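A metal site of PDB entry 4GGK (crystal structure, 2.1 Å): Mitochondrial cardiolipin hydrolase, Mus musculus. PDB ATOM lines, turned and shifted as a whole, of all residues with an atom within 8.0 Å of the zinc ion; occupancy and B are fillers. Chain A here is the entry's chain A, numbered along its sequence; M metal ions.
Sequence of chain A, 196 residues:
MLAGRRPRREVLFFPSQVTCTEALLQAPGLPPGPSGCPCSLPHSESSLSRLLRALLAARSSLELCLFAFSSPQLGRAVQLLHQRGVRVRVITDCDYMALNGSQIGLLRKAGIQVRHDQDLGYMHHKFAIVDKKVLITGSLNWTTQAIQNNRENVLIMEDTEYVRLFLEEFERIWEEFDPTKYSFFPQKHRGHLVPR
The backbone carbonyl oxygen of Leu 41 sits at hydrogen-bond distance from a ring nitrogen (ND1) of His 43 (3.1 Å).
The backbone NH (N) of Glu 22 sits close to the side-chain sulfur (SG) of Cys 20, 3.7 Å away.
N of Cys 20 lies within hydrogen-bond range of O of Pro 42, 3.0 Å away.
SG of Cys 39 sits close to N of Leu 41.
Four residues have an atom within 4 Å of the zinc ion: Cys 20, Cys 37, Cys 39 and His 43.
The zinc ion is bound by NE2 of His 43, at 2.1 Å.
The side-chain sulfur (SG) of Cys 20 is bound to the zinc ion.
SG of Cys 37 binds the zinc ion (2.3 Å).
SG of Cys 39 binds the zinc ion (2.4 Å).
The zinc ion has four donor atoms within binding distance.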
ATOM      1  N   THR A  19      16.472   9.239 -19.177  1.00  0.00           N
ATOM      2  CA  THR A  19      17.226   9.131 -20.426  1.00  0.00           C
ATOM      3  C   THR A  19      16.833  10.233 -21.383  1.00  0.00           C
ATOM      4  O   THR A  19      15.767  10.807 -21.268  1.00  0.00           O
ATOM      5  CB  THR A  19      17.056   7.760 -21.142  1.00  0.00           C
ATOM      6  OG1 THR A  19      15.686   7.542 -21.488  1.00  0.00           O
ATOM      7  CG2 THR A  19      17.569   6.618 -20.274  1.00  0.00           C
ATOM      8  N   CYS A  20      17.719  10.551 -22.317  1.00  0.00           N
ATOM      9  CA  CYS A  20      17.465  11.594 -23.315  1.00  0.00           C
ATOM     10  C   CYS A  20      16.367  11.204 -24.315  1.00  0.00           C
ATOM     11  O   CYS A  20      16.392  10.108 -24.885  1.00  0.00           O
ATOM     12  CB  CYS A  20      18.741  11.866 -24.091  1.00  0.00           C
ATOM     13  SG  CYS A  20      18.618  13.265 -25.180  1.00  0.00           S
ATOM     14  N   THR A  21      15.446  12.136 -24.562  1.00  0.00           N
ATOM     15  CA  THR A  21      14.374  11.937 -25.527  1.00  0.00           C
ATOM     16  C   THR A  21      14.250  13.103 -26.533  1.00  0.00           C
ATOM     17  O   THR A  21      13.204  13.277 -27.146  1.00  0.00           O
ATOM     18  CB  THR A  21      13.022  11.759 -24.793  1.00  0.00           C
ATOM     19  OG1 THR A  21      12.605  13.011 -24.226  1.00  0.00           O
ATOM     20  CG2 THR A  21      13.137  10.678 -23.679  1.00  0.00           C
ATOM     21  N   GLU A  22      15.325  13.878 -26.706  1.00  0.00           N
ATOM     22  CA  GLU A  22      15.300  15.012 -27.634  1.00  0.00           C
ATOM     23  C   GLU A  22      15.011  14.559 -29.064  1.00  0.00           C
ATOM     24  O   GLU A  22      14.105  15.087 -29.733  1.00  0.00           O
ATOM     25  CB  GLU A  22      16.613  15.815 -27.582  1.00  0.00           C
ATOM     26  CG  GLU A  22      16.859  16.597 -26.254  1.00  0.00           C
ATOM     27  CD  GLU A  22      15.668  17.460 -25.809  1.00  0.00           C
ATOM     28  OE1 GLU A  22      15.330  18.449 -26.489  1.00  0.00           O
ATOM     29  OE2 GLU A  22      15.065  17.154 -24.747  1.00  0.00           O
ATOM     30  N   ALA A  23      15.758  13.552 -29.541  1.00  0.00           N
ATOM     31  CA  ALA A  23      15.570  13.040 -30.904  1.00  0.00           C
ATOM     32  C   ALA A  23      14.150  12.522 -31.111  1.00  0.00           C
ATOM     33  O   ALA A  23      13.453  12.960 -32.036  1.00  0.00           O
ATOM     34  CB  ALA A  23      16.596  11.949 -31.227  1.00  0.00           C
ATOM     35  N   CYS A  37      24.036  13.393 -29.603  1.00  0.00           N
ATOM     36  CA  CYS A  37      23.483  14.595 -29.006  1.00  0.00           C
ATOM     37  C   CYS A  37      24.411  15.112 -27.892  1.00  0.00           C
ATOM     38  O   CYS A  37      24.999  14.311 -27.145  1.00  0.00           O
ATOM     39  CB  CYS A  37      22.066  14.310 -28.492  1.00  0.00           C
ATOM     40  SG  CYS A  37      21.469  15.306 -27.098  1.00  0.00           S
ATOM     41  N   PRO A  38      24.558  16.450 -27.796  1.00  0.00           N
ATOM     42  CA  PRO A  38      25.512  17.052 -26.850  1.00  0.00           C
ATOM     43  C   PRO A  38      25.139  16.957 -25.363  1.00  0.00           C
ATOM     44  O   PRO A  38      26.002  17.196 -24.505  1.00  0.00           O
ATOM     45  CB  PRO A  38      25.573  18.520 -27.298  1.00  0.00           C
ATOM     46  CG  PRO A  38      24.275  18.768 -27.973  1.00  0.00           C
ATOM     47  CD  PRO A  38      23.895  17.472 -28.626  1.00  0.00           C
ATOM     48  N   CYS A  39      23.886  16.626 -25.050  1.00  0.00           N
ATOM     49  CA  CYS A  39      23.441  16.561 -23.659  1.00  0.00           C
ATOM     50  C   CYS A  39      24.133  15.425 -22.899  1.00  0.00           C
ATOM     51  O   CYS A  39      24.802  14.575 -23.484  1.00  0.00           O
ATOM     52  CB  CYS A  39      21.927  16.384 -23.562  1.00  0.00           C
ATOM     53  SG  CYS A  39      21.429  14.701 -23.271  1.00  0.00           S
ATOM     54  N   SER A  40      23.933  15.434 -21.583  1.00  0.00           N
ATOM     55  CA  SER A  40      24.709  14.613 -20.655  1.00  0.00           C
ATOM     56  C   SER A  40      23.965  13.397 -20.146  1.00  0.00           C
ATOM     57  O   SER A  40      24.501  12.645 -19.339  1.00  0.00           O
ATOM     58  CB  SER A  40      25.126  15.472 -19.455  1.00  0.00           C
ATOM     59  OG  SER A  40      25.830  16.637 -19.872  1.00  0.00           O
ATOM     60  N   LEU A  41      22.736  13.190 -20.618  1.00  0.00           N
ATOM     61  CA  LEU A  41      21.944  12.036 -20.220  1.00  0.00           C
ATOM     62  C   LEU A  41      22.365  10.781 -20.985  1.00  0.00           C
ATOM     63  O   LEU A  41      22.997  10.868 -22.034  1.00  0.00           O
ATOM     64  CB  LEU A  41      20.442  12.295 -20.432  1.00  0.00           C
ATOM     65  CG  LEU A  41      19.803  13.325 -19.484  1.00  0.00           C
ATOM     66  CD1 LEU A  41      18.305  13.438 -19.751  1.00  0.00           C
ATOM     67  CD2 LEU A  41      20.048  12.935 -18.033  1.00  0.00           C
ATOM     68  N   PRO A  42      21.995   9.599 -20.459  1.00  0.00           N
ATOM     69  CA  PRO A  42      22.170   8.341 -21.180  1.00  0.00           C
ATOM     70  C   PRO A  42      21.279   8.336 -22.413  1.00  0.00           C
ATOM     71  O   PRO A  42      20.117   8.720 -22.297  1.00  0.00           O
ATOM     72  CB  PRO A  42      21.651   7.274 -20.190  1.00  0.00           C
ATOM     73  CG  PRO A  42      21.557   7.961 -18.869  1.00  0.00           C
ATOM     74  CD  PRO A  42      21.338   9.403 -19.157  1.00  0.00           C
ATOM     75  N   HIS A  43      21.799   7.908 -23.555  1.00  0.00           N
ATOM     76  CA  HIS A  43      20.977   7.850 -24.776  1.00  0.00           C
ATOM     77  C   HIS A  43      20.520   6.436 -25.100  1.00  0.00           C
ATOM     78  O   HIS A  43      20.715   5.929 -26.199  1.00  0.00           O
ATOM     79  CB  HIS A  43      21.731   8.451 -25.942  1.00  0.00           C
ATOM     80  CG  HIS A  43      21.951   9.927 -25.808  1.00  0.00           C
ATOM     81  ND1 HIS A  43      23.019  10.459 -25.116  1.00  0.00           N
ATOM     82  CD2 HIS A  43      21.235  10.975 -26.273  1.00  0.00           C
ATOM     83  CE1 HIS A  43      22.960  11.776 -25.164  1.00  0.00           C
ATOM     84  NE2 HIS A  43      21.873  12.115 -25.859  1.00  0.00           N
HETATM   85 ZN    ZN M   1      20.827  13.856 -25.381  1.00  0.00          ZN
